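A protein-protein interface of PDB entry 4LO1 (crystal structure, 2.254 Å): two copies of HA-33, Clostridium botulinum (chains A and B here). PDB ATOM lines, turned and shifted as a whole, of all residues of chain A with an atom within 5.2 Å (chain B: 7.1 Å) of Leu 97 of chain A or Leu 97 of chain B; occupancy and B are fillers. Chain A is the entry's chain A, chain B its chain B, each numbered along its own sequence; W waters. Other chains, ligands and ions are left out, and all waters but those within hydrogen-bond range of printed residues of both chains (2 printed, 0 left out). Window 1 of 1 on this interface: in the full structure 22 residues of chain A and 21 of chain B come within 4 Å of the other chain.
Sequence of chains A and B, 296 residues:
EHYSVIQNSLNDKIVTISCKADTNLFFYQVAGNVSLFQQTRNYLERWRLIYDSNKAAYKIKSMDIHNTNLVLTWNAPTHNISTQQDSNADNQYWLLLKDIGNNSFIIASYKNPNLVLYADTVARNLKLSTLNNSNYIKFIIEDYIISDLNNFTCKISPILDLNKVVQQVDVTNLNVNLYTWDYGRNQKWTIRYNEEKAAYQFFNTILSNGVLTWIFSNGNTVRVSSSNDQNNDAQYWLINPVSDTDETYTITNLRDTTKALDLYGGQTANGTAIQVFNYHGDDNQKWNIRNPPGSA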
ATOM      1  N   LEU A  95     -18.458 -11.185  11.276  1.00  0.00           N
ATOM      2  CA  LEU A  95     -17.497 -12.242  11.013  1.00  0.00           C
ATOM      3  C   LEU A  95     -17.772 -12.793   9.628  1.00  0.00           C
ATOM      4  O   LEU A  95     -18.889 -13.210   9.326  1.00  0.00           O
ATOM      5  CB  LEU A  95     -17.619 -13.367  12.047  1.00  0.00           C
ATOM      6  CG  LEU A  95     -17.608 -13.004  13.536  1.00  0.00           C
ATOM      7  CD1 LEU A  95     -17.658 -14.272  14.391  1.00  0.00           C
ATOM      8  CD2 LEU A  95     -16.401 -12.145  13.894  1.00  0.00           C
ATOM      9  N   LEU A  96     -16.756 -12.777   8.778  1.00  0.00           N
ATOM     10  CA  LEU A  96     -16.876 -13.364   7.454  1.00  0.00           C
ATOM     11  C   LEU A  96     -16.340 -14.784   7.511  1.00  0.00           C
ATOM     12  O   LEU A  96     -15.131 -15.002   7.567  1.00  0.00           O
ATOM     13  CB  LEU A  96     -16.113 -12.532   6.421  1.00  0.00           C
ATOM     14  CG  LEU A  96     -16.507 -11.053   6.395  1.00  0.00           C
ATOM     15  CD1 LEU A  96     -15.819 -10.323   5.250  1.00  0.00           C
ATOM     16  CD2 LEU A  96     -18.020 -10.894   6.317  1.00  0.00           C
ATOM     17  N   LEU A  97     -17.250 -15.748   7.520  1.00  0.00           N
ATOM     18  CA  LEU A  97     -16.874 -17.147   7.660  1.00  0.00           C
ATOM     19  C   LEU A  97     -17.040 -17.840   6.321  1.00  0.00           C
ATOM     20  O   LEU A  97     -18.158 -18.026   5.845  1.00  0.00           O
ATOM     21  CB  LEU A  97     -17.747 -17.821   8.720  1.00  0.00           C
ATOM     22  CG  LEU A  97     -17.861 -17.054  10.042  1.00  0.00           C
ATOM     23  CD1 LEU A  97     -18.867 -17.712  10.986  1.00  0.00           C
ATOM     24  CD2 LEU A  97     -16.493 -16.923  10.705  1.00  0.00           C
ATOM     25  N   LYS A  98     -15.927 -18.210   5.705  1.00  0.00           N
ATOM     26  CA  LYS A  98     -15.979 -18.793   4.371  1.00  0.00           C
ATOM     27  C   LYS A  98     -16.299 -20.284   4.418  1.00  0.00           C
ATOM     28  O   LYS A  98     -15.567 -21.074   5.015  1.00  0.00           O
ATOM     29  CB  LYS A  98     -14.670 -18.540   3.617  1.00  0.00           C
ATOM     30  CG  LYS A  98     -14.772 -18.758   2.111  1.00  0.00           C
ATOM     31  CD  LYS A  98     -13.467 -18.402   1.421  1.00  0.00           C
ATOM     32  CE  LYS A  98     -13.577 -18.533  -0.088  1.00  0.00           C
ATOM     33  NZ  LYS A  98     -12.289 -18.211  -0.760  1.00  0.00           N
ATOM     34  N   ASP A  99     -17.407 -20.656   3.789  1.00  0.00           N
ATOM     35  CA  ASP A  99     -17.802 -22.052   3.701  1.00  0.00           C
ATOM     36  C   ASP A  99     -16.978 -22.719   2.606  1.00  0.00           C
ATOM     37  O   ASP A  99     -17.342 -22.681   1.430  1.00  0.00           O
ATOM     38  CB  ASP A  99     -19.293 -22.157   3.390  1.00  0.00           C
ATOM     39  CG  ASP A  99     -19.845 -23.549   3.622  1.00  0.00           C
ATOM     40  OD1 ASP A  99     -19.069 -24.526   3.577  1.00  0.00           O
ATOM     41  OD2 ASP A  99     -21.065 -23.664   3.851  1.00  0.00           O
ATOM     42  N   ILE A 100     -15.863 -23.324   3.002  1.00  0.00           N
ATOM     43  CA  ILE A 100     -14.909 -23.879   2.049  1.00  0.00           C
ATOM     44  C   ILE A 100     -15.523 -25.003   1.225  1.00  0.00           C
ATOM     45  O   ILE A 100     -16.223 -25.866   1.753  1.00  0.00           O
ATOM     46  CB  ILE A 100     -13.639 -24.385   2.755  1.00  0.00           C
ATOM     47  CG1 ILE A 100     -13.027 -23.263   3.590  1.00  0.00           C
ATOM     48  CG2 ILE A 100     -12.623 -24.887   1.741  1.00  0.00           C
ATOM     49  CD1 ILE A 100     -12.669 -22.037   2.780  1.00  0.00           C
ATOM     50  N   SER A 104     -19.000 -19.769  -0.626  1.00  0.00           N
ATOM     51  CA  SER A 104     -19.990 -18.845  -0.102  1.00  0.00           C
ATOM     52  C   SER A 104     -19.590 -18.444   1.308  1.00  0.00           C
ATOM     53  O   SER A 104     -18.744 -19.090   1.929  1.00  0.00           O
ATOM     54  CB  SER A 104     -21.377 -19.487  -0.097  1.00  0.00           C
ATOM     55  OG  SER A 104     -21.429 -20.585   0.794  1.00  0.00           O
ATOM     56  N   PHE A 105     -20.193 -17.373   1.807  1.00  0.00           N
ATOM     57  CA  PHE A 105     -19.894 -16.882   3.142  1.00  0.00           C
ATOM     58  C   PHE A 105     -21.125 -16.930   4.031  1.00  0.00           C
ATOM     59  O   PHE A 105     -22.240 -16.638   3.594  1.00  0.00           O
ATOM     60  CB  PHE A 105     -19.384 -15.436   3.094  1.00  0.00           C
ATOM     61  CG  PHE A 105     -17.965 -15.299   2.609  1.00  0.00           C
ATOM     62  CD1 PHE A 105     -16.924 -15.136   3.510  1.00  0.00           C
ATOM     63  CD2 PHE A 105     -17.676 -15.311   1.254  1.00  0.00           C
ATOM     64  CE1 PHE A 105     -15.619 -15.001   3.070  1.00  0.00           C
ATOM     65  CE2 PHE A 105     -16.368 -15.175   0.804  1.00  0.00           C
ATOM     66  CZ  PHE A 105     -15.340 -15.020   1.713  1.00  0.00           C
ATOM     67  N   ILE A 106     -20.908 -17.314   5.281  1.00  0.00           N
ATOM     68  CA  ILE A 106     -21.870 -17.052   6.330  1.00  0.00           C
ATOM     69  C   ILE A 106     -21.385 -15.801   7.049  1.00  0.00           C
ATOM     70  O   ILE A 106     -20.215 -15.696   7.413  1.00  0.00           O
ATOM     71  CB  ILE A 106     -21.986 -18.230   7.311  1.00  0.00           C
ATOM     72  CG1 ILE A 106     -22.620 -19.435   6.614  1.00  0.00           C
ATOM     73  CG2 ILE A 106     -22.815 -17.823   8.524  1.00  0.00           C
ATOM     74  CD1 ILE A 106     -22.854 -20.632   7.537  1.00  0.00           C
ATOM     75  N   ILE A 107     -22.276 -14.837   7.222  1.00  0.00           N
ATOM     76  CA  ILE A 107     -21.890 -13.549   7.777  1.00  0.00           C
ATOM     77  C   ILE A 107     -22.529 -13.385   9.149  1.00  0.00           C
ATOM     78  O   ILE A 107     -23.721 -13.096   9.260  1.00  0.00           O
ATOM     79  CB  ILE A 107     -22.297 -12.394   6.830  1.00  0.00           C
ATOM     80  CG1 ILE A 107     -21.694 -12.620   5.440  1.00  0.00           C
ATOM     81  CG2 ILE A 107     -21.864 -11.043   7.390  1.00  0.00           C
ATOM     82  CD1 ILE A 107     -22.068 -11.554   4.416  1.00  0.00           C
ATOM     83  N   ALA A 108     -21.733 -13.593  10.193  1.00  0.00           N
ATOM     84  CA  ALA A 108     -22.246 -13.602  11.556  1.00  0.00           C
ATOM     85  C   ALA A 108     -22.017 -12.267  12.248  1.00  0.00           C
ATOM     86  O   ALA A 108     -21.002 -11.608  12.023  1.00  0.00           O
ATOM     87  CB  ALA A 108     -21.596 -14.728  12.360  1.00  0.00           C
ATOM     88  N   ALA B  56     -22.546 -29.980   1.131  1.00  0.00           N
ATOM     89  CA  ALA B  56     -21.567 -28.914   1.330  1.00  0.00           C
ATOM     90  C   ALA B  56     -20.924 -29.025   2.710  1.00  0.00           C
ATOM     91  O   ALA B  56     -20.710 -28.023   3.395  1.00  0.00           O
ATOM     92  CB  ALA B  56     -22.198 -27.536   1.126  1.00  0.00           C
ATOM     93  N   TYR B  58     -18.212 -31.825   5.390  1.00  0.00           N
ATOM     94  CA  TYR B  58     -17.083 -32.749   5.393  1.00  0.00           C
ATOM     95  C   TYR B  58     -17.197 -33.822   6.465  1.00  0.00           C
ATOM     96  O   TYR B  58     -17.655 -33.561   7.580  1.00  0.00           O
ATOM     97  CB  TYR B  58     -15.777 -31.994   5.639  1.00  0.00           C
ATOM     98  CG  TYR B  58     -15.387 -31.028   4.550  1.00  0.00           C
ATOM     99  CD1 TYR B  58     -14.464 -31.386   3.574  1.00  0.00           C
ATOM    100  CD2 TYR B  58     -15.932 -29.751   4.501  1.00  0.00           C
ATOM    101  CE1 TYR B  58     -14.099 -30.500   2.577  1.00  0.00           C
ATOM    102  CE2 TYR B  58     -15.576 -28.861   3.514  1.00  0.00           C
ATOM    103  CZ  TYR B  58     -14.659 -29.238   2.554  1.00  0.00           C
ATOM    104  OH  TYR B  58     -14.313 -28.344   1.570  1.00  0.00           O
ATOM    105  N   TRP B  94     -19.578 -32.154   8.988  1.00  0.00           N
ATOM    106  CA  TRP B  94     -19.179 -30.895   9.605  1.00  0.00           C
ATOM    107  C   TRP B  94     -18.988 -29.798   8.569  1.00  0.00           C
ATOM    108  O   TRP B  94     -18.451 -30.040   7.487  1.00  0.00           O
ATOM    109  CB  TRP B  94     -17.880 -31.087  10.390  1.00  0.00           C
ATOM    110  CG  TRP B  94     -17.992 -32.160  11.417  1.00  0.00           C
ATOM    111  CD1 TRP B  94     -17.732 -33.489  11.248  1.00  0.00           C
ATOM    112  CD2 TRP B  94     -18.420 -32.001  12.773  1.00  0.00           C
ATOM    113  NE1 TRP B  94     -17.965 -34.167  12.418  1.00  0.00           N
ATOM    114  CE2 TRP B  94     -18.389 -33.277  13.370  1.00  0.00           C
ATOM    115  CE3 TRP B  94     -18.823 -30.906  13.542  1.00  0.00           C
ATOM    116  CZ2 TRP B  94     -18.745 -33.487  14.701  1.00  0.00           C
ATOM    117  CZ3 TRP B  94     -19.180 -31.118  14.866  1.00  0.00           C
ATOM    118  CH2 TRP B  94     -19.137 -32.398  15.430  1.00  0.00           C
ATOM    119  N   LEU B  95     -19.433 -28.593   8.904  1.00  0.00           N
ATOM    120  CA  LEU B  95     -19.185 -27.435   8.061  1.00  0.00           C
ATOM    121  C   LEU B  95     -17.836 -26.853   8.446  1.00  0.00           C
ATOM    122  O   LEU B  95     -17.584 -26.579   9.620  1.00  0.00           O
ATOM    123  CB  LEU B  95     -20.274 -26.374   8.247  1.00  0.00           C
ATOM    124  CG  LEU B  95     -21.746 -26.781   8.158  1.00  0.00           C
ATOM    125  CD1 LEU B  95     -22.615 -25.539   8.057  1.00  0.00           C
ATOM    126  CD2 LEU B  95     -21.989 -27.702   6.983  1.00  0.00           C
ATOM    127  N   LEU B  96     -16.961 -26.685   7.462  1.00  0.00           N
ATOM    128  CA  LEU B  96     -15.659 -26.085   7.713  1.00  0.00           C
ATOM    129  C   LEU B  96     -15.695 -24.618   7.315  1.00  0.00           C
ATOM    130  O   LEU B  96     -15.551 -24.273   6.142  1.00  0.00           O
ATOM    131  CB  LEU B  96     -14.560 -26.825   6.949  1.00  0.00           C
ATOM    132  CG  LEU B  96     -14.381 -28.310   7.298  1.00  0.00           C
ATOM    133  CD1 LEU B  96     -13.194 -28.893   6.554  1.00  0.00           C
ATOM    134  CD2 LEU B  96     -14.234 -28.521   8.799  1.00  0.00           C
ATOM    135  N   LEU B  97     -15.899 -23.759   8.303  1.00  0.00           N
ATOM    136  CA  LEU B  97     -16.029 -22.332   8.059  1.00  0.00           C
ATOM    137  C   LEU B  97     -14.722 -21.628   8.383  1.00  0.00           C
ATOM    138  O   LEU B  97     -14.318 -21.562   9.545  1.00  0.00           O
ATOM    139  CB  LEU B  97     -17.153 -21.760   8.921  1.00  0.00           C
ATOM    140  CG  LEU B  97     -18.462 -22.546   8.862  1.00  0.00           C
ATOM    141  CD1 LEU B  97     -19.504 -21.942   9.801  1.00  0.00           C
ATOM    142  CD2 LEU B  97     -18.979 -22.607   7.428  1.00  0.00           C
ATOM    143  N   LYS B  98     -14.064 -21.098   7.357  1.00  0.00           N
ATOM    144  CA  LYS B  98     -12.800 -20.406   7.551  1.00  0.00           C
ATOM    145  C   LYS B  98     -13.019 -18.941   7.925  1.00  0.00           C
ATOM    146  O   LYS B  98     -13.589 -18.171   7.153  1.00  0.00           O
ATOM    147  CB  LYS B  98     -11.938 -20.508   6.294  1.00  0.00           C
ATOM    148  CG  LYS B  98     -10.494 -20.090   6.499  1.00  0.00           C
ATOM    149  CD  LYS B  98      -9.673 -20.338   5.247  1.00  0.00           C
ATOM    150  CE  LYS B  98      -8.212 -19.986   5.464  1.00  0.00           C
ATOM    151  NZ  LYS B  98      -7.404 -20.189   4.227  1.00  0.00           N
ATOM    152  N   ASP B  99     -12.569 -18.565   9.118  1.00  0.00           N
ATOM    153  CA  ASP B  99     -12.648 -17.177   9.561  1.00  0.00           C
ATOM    154  C   ASP B  99     -11.564 -16.357   8.868  1.00  0.00           C
ATOM    155  O   ASP B  99     -10.419 -16.328   9.319  1.00  0.00           O
ATOM    156  CB  ASP B  99     -12.482 -17.103  11.080  1.00  0.00           C
ATOM    157  CG  ASP B  99     -12.819 -15.733  11.648  1.00  0.00           C
ATOM    158  OD1 ASP B  99     -12.862 -14.743  10.885  1.00  0.00           O
ATOM    159  OD2 ASP B  99     -13.036 -15.649  12.873  1.00  0.00           O
ATOM    160  N   ILE B 100     -11.926 -15.688   7.776  1.00  0.00           N
ATOM    161  CA  ILE B 100     -10.946 -14.952   6.975  1.00  0.00           C
ATOM    162  C   ILE B 100     -10.294 -13.806   7.749  1.00  0.00           C
ATOM    163  O   ILE B 100     -10.950 -13.104   8.518  1.00  0.00           O
ATOM    164  CB  ILE B 100     -11.557 -14.422   5.657  1.00  0.00           C
ATOM    165  CG1 ILE B 100     -12.248 -15.557   4.903  1.00  0.00           C
ATOM    166  CG2 ILE B 100     -10.481 -13.812   4.772  1.00  0.00           C
ATOM    167  CD1 ILE B 100     -11.296 -16.617   4.407  1.00  0.00           C
ATOM    168  N   SER B 104      -8.118 -19.196  10.847  1.00  0.00           N
ATOM    169  CA  SER B 104      -8.591 -20.273  11.704  1.00  0.00           C
ATOM    170  C   SER B 104      -9.935 -20.780  11.199  1.00  0.00           C
ATOM    171  O   SER B 104     -10.568 -20.147  10.353  1.00  0.00           O
ATOM    172  CB  SER B 104      -8.711 -19.797  13.152  1.00  0.00           C
ATOM    173  OG  SER B 104      -9.672 -18.763  13.269  1.00  0.00           O
ATOM    174  N   PHE B 105     -10.366 -21.923  11.723  1.00  0.00           N
ATOM    175  CA  PHE B 105     -11.612 -22.543  11.296  1.00  0.00           C
ATOM    176  C   PHE B 105     -12.597 -22.695  12.441  1.00  0.00           C
ATOM    177  O   PHE B 105     -12.221 -23.032  13.563  1.00  0.00           O
ATOM    178  CB  PHE B 105     -11.346 -23.932  10.709  1.00  0.00           C
ATOM    179  CG  PHE B 105     -10.867 -23.918   9.287  1.00  0.00           C
ATOM    180  CD1 PHE B 105     -11.769 -24.017   8.238  1.00  0.00           C
ATOM    181  CD2 PHE B 105      -9.515 -23.826   9.000  1.00  0.00           C
ATOM    182  CE1 PHE B 105     -11.329 -24.013   6.927  1.00  0.00           C
ATOM    183  CE2 PHE B 105      -9.067 -23.822   7.692  1.00  0.00           C
ATOM    184  CZ  PHE B 105      -9.976 -23.914   6.653  1.00  0.00           C
ATOM    185  N   ILE B 106     -13.864 -22.445  12.139  1.00  0.00           N
ATOM    186  CA  ILE B 106     -14.952 -22.845  13.010  1.00  0.00           C
ATOM    187  C   ILE B 106     -15.520 -24.117  12.406  1.00  0.00           C
ATOM    188  O   ILE B 106     -15.731 -24.196  11.194  1.00  0.00           O
ATOM    189  CB  ILE B 106     -16.042 -21.756  13.091  1.00  0.00           C
ATOM    190  CG1 ILE B 106     -15.507 -20.538  13.841  1.00  0.00           C
ATOM    191  CG2 ILE B 106     -17.289 -22.293  13.770  1.00  0.00           C
ATOM    192  CD1 ILE B 106     -16.529 -19.448  14.043  1.00  0.00           C
ATOM    193  N   ILE B 107     -15.740 -25.123  13.244  1.00  0.00           N
ATOM    194  CA  ILE B 107     -16.203 -26.419  12.765  1.00  0.00           C
ATOM    195  C   ILE B 107     -17.604 -26.715  13.286  1.00  0.00           C
ATOM    196  O   ILE B 107     -17.779 -27.162  14.422  1.00  0.00           O
ATOM    197  CB  ILE B 107     -15.225 -27.542  13.174  1.00  0.00           C
ATOM    198  CG1 ILE B 107     -13.809 -27.205  12.697  1.00  0.00           C
ATOM    199  CG2 ILE B 107     -15.672 -28.879  12.601  1.00  0.00           C
ATOM    200  CD1 ILE B 107     -12.759 -28.205  13.127  1.00  0.00           C
ATOM    201  N   ALA B 108     -18.599 -26.459  12.444  1.00  0.00           N
ATOM    202  CA  ALA B 108     -19.997 -26.544  12.845  1.00  0.00           C
ATOM    203  C   ALA B 108     -20.627 -27.882  12.468  1.00  0.00           C
ATOM    204  O   ALA B 108     -20.367 -28.415  11.390  1.00  0.00           O
ATOM    205  CB  ALA B 108     -20.792 -25.387  12.219  1.00  0.00           C
ATOM    206  N   PRO B 113     -26.204 -26.852  12.869  1.00  0.00           N
ATOM    207  CA  PRO B 113     -25.269 -25.765  12.551  1.00  0.00           C
ATOM    208  C   PRO B 113     -25.154 -24.712  13.654  1.00  0.00           C
ATOM    209  O   PRO B 113     -24.215 -23.920  13.634  1.00  0.00           O
ATOM    210  CB  PRO B 113     -25.876 -25.142  11.291  1.00  0.00           C
ATOM    211  CG  PRO B 113     -26.695 -26.221  10.687  1.00  0.00           C
ATOM    212  CD  PRO B 113     -27.238 -27.010  11.833  1.00  0.00           C
ATOM    213  N   VAL B 116     -21.038 -25.823  17.361  1.00  0.00           N
ATOM    214  CA  VAL B 116     -19.707 -25.932  16.784  1.00  0.00           C
ATOM    215  C   VAL B 116     -18.770 -26.578  17.795  1.00  0.00           C
ATOM    216  O   VAL B 116     -19.067 -26.607  18.990  1.00  0.00           O
ATOM    217  CB  VAL B 116     -19.151 -24.551  16.371  1.00  0.00           C
ATOM    218  CG1 VAL B 116     -20.159 -23.812  15.507  1.00  0.00           C
ATOM    219  CG2 VAL B 116     -18.807 -23.723  17.594  1.00  0.00           C
ATOM    220  N   LEU B 131     -22.154 -20.334  18.757  1.00  0.00           N
ATOM    221  CA  LEU B 131     -21.072 -19.462  18.309  1.00  0.00           C
ATOM    222  C   LEU B 131     -20.814 -18.283  19.234  1.00  0.00           C
ATOM    223  O   LEU B 131     -21.741 -17.695  19.784  1.00  0.00           O
ATOM    224  CB  LEU B 131     -21.330 -18.951  16.896  1.00  0.00           C
ATOM    225  CG  LEU B 131     -21.009 -19.935  15.781  1.00  0.00           C
ATOM    226  CD1 LEU B 131     -22.219 -20.795  15.495  1.00  0.00           C
ATOM    227  CD2 LEU B 131     -20.565 -19.187  14.545  1.00  0.00           C
ATOM    228  N   LYS B 138     -12.156 -21.919  17.760  1.00  0.00           N
ATOM    229  CA  LYS B 138     -11.355 -21.720  16.561  1.00  0.00           C
ATOM    230  C   LYS B 138     -10.251 -22.763  16.466  1.00  0.00           C
ATOM    231  O   LYS B 138      -9.591 -23.076  17.455  1.00  0.00           O
ATOM    232  CB  LYS B 138     -10.758 -20.314  16.528  1.00  0.00           C
ATOM    233  CG  LYS B 138     -11.780 -19.212  16.340  1.00  0.00           C
ATOM    234  CD  LYS B 138     -11.080 -17.883  16.121  1.00  0.00           C
ATOM    235  CE  LYS B 138     -12.058 -16.787  15.714  1.00  0.00           C
ATOM    236  NZ  LYS B 138     -12.870 -16.283  16.863  1.00  0.00           N
ATOM    237  N   PHE B 139     -10.048 -23.290  15.264  1.00  0.00           N
ATOM    238  CA  PHE B 139      -9.097 -24.373  15.060  1.00  0.00           C
ATOM    239  C   PHE B 139      -8.203 -24.131  13.851  1.00  0.00           C
ATOM    240  O   PHE B 139      -8.609 -23.503  12.874  1.00  0.00           O
ATOM    241  CB  PHE B 139      -9.841 -25.702  14.919  1.00  0.00           C
ATOM    242  CG  PHE B 139     -10.679 -26.053  16.119  1.00  0.00           C
ATOM    243  CD1 PHE B 139     -10.121 -26.723  17.197  1.00  0.00           C
ATOM    244  CD2 PHE B 139     -12.018 -25.700  16.174  1.00  0.00           C
ATOM    245  CE1 PHE B 139     -10.884 -27.040  18.308  1.00  0.00           C
ATOM    246  CE2 PHE B 139     -12.787 -26.014  17.280  1.00  0.00           C
ATOM    247  CZ  PHE B 139     -12.218 -26.688  18.351  1.00  0.00           C
ATOM    248  N   ILE B 141      -6.411 -25.801  10.863  1.00  0.00           N
ATOM    249  CA  ILE B 141      -6.379 -26.968   9.992  1.00  0.00           C
ATOM    250  C   ILE B 141      -5.220 -26.834   9.026  1.00  0.00           C
ATOM    251  O   ILE B 141      -5.158 -25.880   8.255  1.00  0.00           O
ATOM    252  CB  ILE B 141      -7.674 -27.104   9.176  1.00  0.00           C
ATOM    253  CG1 ILE B 141      -8.878 -27.270  10.107  1.00  0.00           C
ATOM    254  CG2 ILE B 141      -7.565 -28.270   8.195  1.00  0.00           C
ATOM    255  CD1 ILE B 141     -10.191 -27.474   9.378  1.00  0.00           C
HETATM  256  O   HOH W   1     -18.247 -26.869   4.707  1.00  0.00           O
HETATM  257  O   HOH W   2     -14.332 -12.324  10.428  1.00  0.00           O
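The backbone NH of Lys 98 of chain A lies within hydrogen-bond range of the backbone carbonyl oxygen of Lys 98 of chain B (2.8 Å).
The backbone carbonyl oxygen (O) of Leu 96 of chain A lies within hydrogen-bond range of the backbone NH (N) of Ile 100 of chain B (3.3 Å).
The backbone carbonyl oxygen (O) of Ile 100 of chain A is in hydrogen-bond range of the side-chain hydroxyl (OH) of Tyr 58 of chain B (3.1 Å).
O of Leu 96 of chain B sits close to O of Lys 98 of chain A (3.4 Å).
The backbone NH (N) of Ile 100 of chain A lies within hydrogen-bond range of the backbone carbonyl oxygen (O) of Leu 96 of chain B.
N of Ile 106 of chain A lies within hydrogen-bond range of O of Leu 97 of chain A, at 2.9 Å.
N of Tyr 58 of chain B is in hydrogen-bond range of O of Trp 94 of chain B (2.8 Å).
N of Asp 99 of chain B is in hydrogen-bond range of O of Ser 104 of chain B, 2.8 Å away.
The backbone NH (N) of Phe 105 of chain B lies within hydrogen-bond range of the backbone carbonyl oxygen (O) of Phe 139 of chain B (2.6 Å).
The backbone carbonyl oxygen of Leu 97 of chain B is in hydrogen-bond range of the backbone NH of Ile 106 of chain B, 2.8 Å away.
The backbone NH (N) of Asp 99 of chain A is in hydrogen-bond range of the backbone carbonyl oxygen (O) of Ser 104 of chain A (2.8 Å).
Among the printed residues, merely in contact across the chains: Leu 96 of chain A with Lys 98 of chain B (3.5 Å), Leu 96 of chain A with Asp 99 of chain B (3.9 Å), Leu 97 of chain A with Leu 97 of chain B (3.99 Å), Leu 97 of chain A with Lys 98 of chain B (3.5 Å), Leu 97 of chain A with Asp 99 of chain B (3.98 Å), Lys 98 of chain A with Leu 97 of chain B (3.3 Å), Lys 98 of chain A with Ile 100 of chain B (3.96 Å), Asp 99 of chain A with Ala 56 of chain B (3.9 Å), Asp 99 of chain A with Leu 96 of chain B (3.99 Å), Asp 99 of chain A with Leu 97 of chain B (3.9 Å), Ile 100 of chain A with Lys 98 of chain B (3.9 Å), Ile 100 of chain A with Phe 105 of chain B (3.8 Å) and Phe 105 of chain A with Ile 100 of chain B (3.9 Å).
Printed residues of chain B within 4 Å of Leu 97 of chain A: Leu 97, Lys 98 and Asp 99.
Printed residues of chain B within 4 Å of Ile 100 of chain A: Tyr 58, Leu 96, Lys 98 and Phe 105.
Printed residues of chain A within 4 Å of Tyr 58 of chain B: Ile 100 (3.1 Å).
Of the printed residues of chain A, Leu 97 of chain B touches Leu 97 (3.99 Å), Lys 98 (3.3 Å) and Asp 99 (3.9 Å).
Of the printed residues of chain A, Lys 98 of chain B touches Leu 96, Leu 97, Lys 98 and Ile 100.
The nearest printed residue of chain B that does not touch Leu 97 of chain A is Ile 106 of chain B (4.2 Å).
The nearest printed residue of chain A that does not touch Lys 98 of chain B is Asp 99 of chain A (4.9 Å).
Hydrophobic or aromatic side chains of chain A that line the printed part of chain B: Leu 97, Ile 100 and Phe 105.
Of the 20 printed residues of chain B, 8 touch a printed residue of chain A.
Printed residues of chain B that touch a printed residue of chain A: Ala 56, Tyr 58, Leu 96, Leu 97, Lys 98, Asp 99, Ile 100 and Phe 105.
Among the printed residues, 18 pairs touch across the chains.
Leu 96 of chain A touches Lys 98 of chain B, and with the chains exchanged Lys 98 of chain A touches Leu 96 of chain B.
Leu 97 of chain A touches Lys 98 of chain B, and with the chains exchanged Lys 98 of chain A touches Leu 97 of chain B.
Leu 97 of chain A touches Asp 99 of chain B, and with the chains exchanged Asp 99 of chain A touches Leu 97 of chain B.
Ile 100 of chain A touches Phe 105 of chain B, and with the chains exchanged Phe 105 of chain A touches Ile 100 of chain B.
11 positions are printed for both chains.
Water W1 lies within hydrogen-bond range of the side-chain carboxylate (OD1) of Asp 99 of chain A (2.7 Å), the backbone carbonyl oxygen (O) of Ala 56 of chain B (3.0 Å) and the backbone NH (N) of Leu 96 of chain B (3.0 Å).
Water W2 bridges OD1 of Asp 99 of chain B (2.9 Å) and N of Leu 96 of chain A (3.0 Å).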
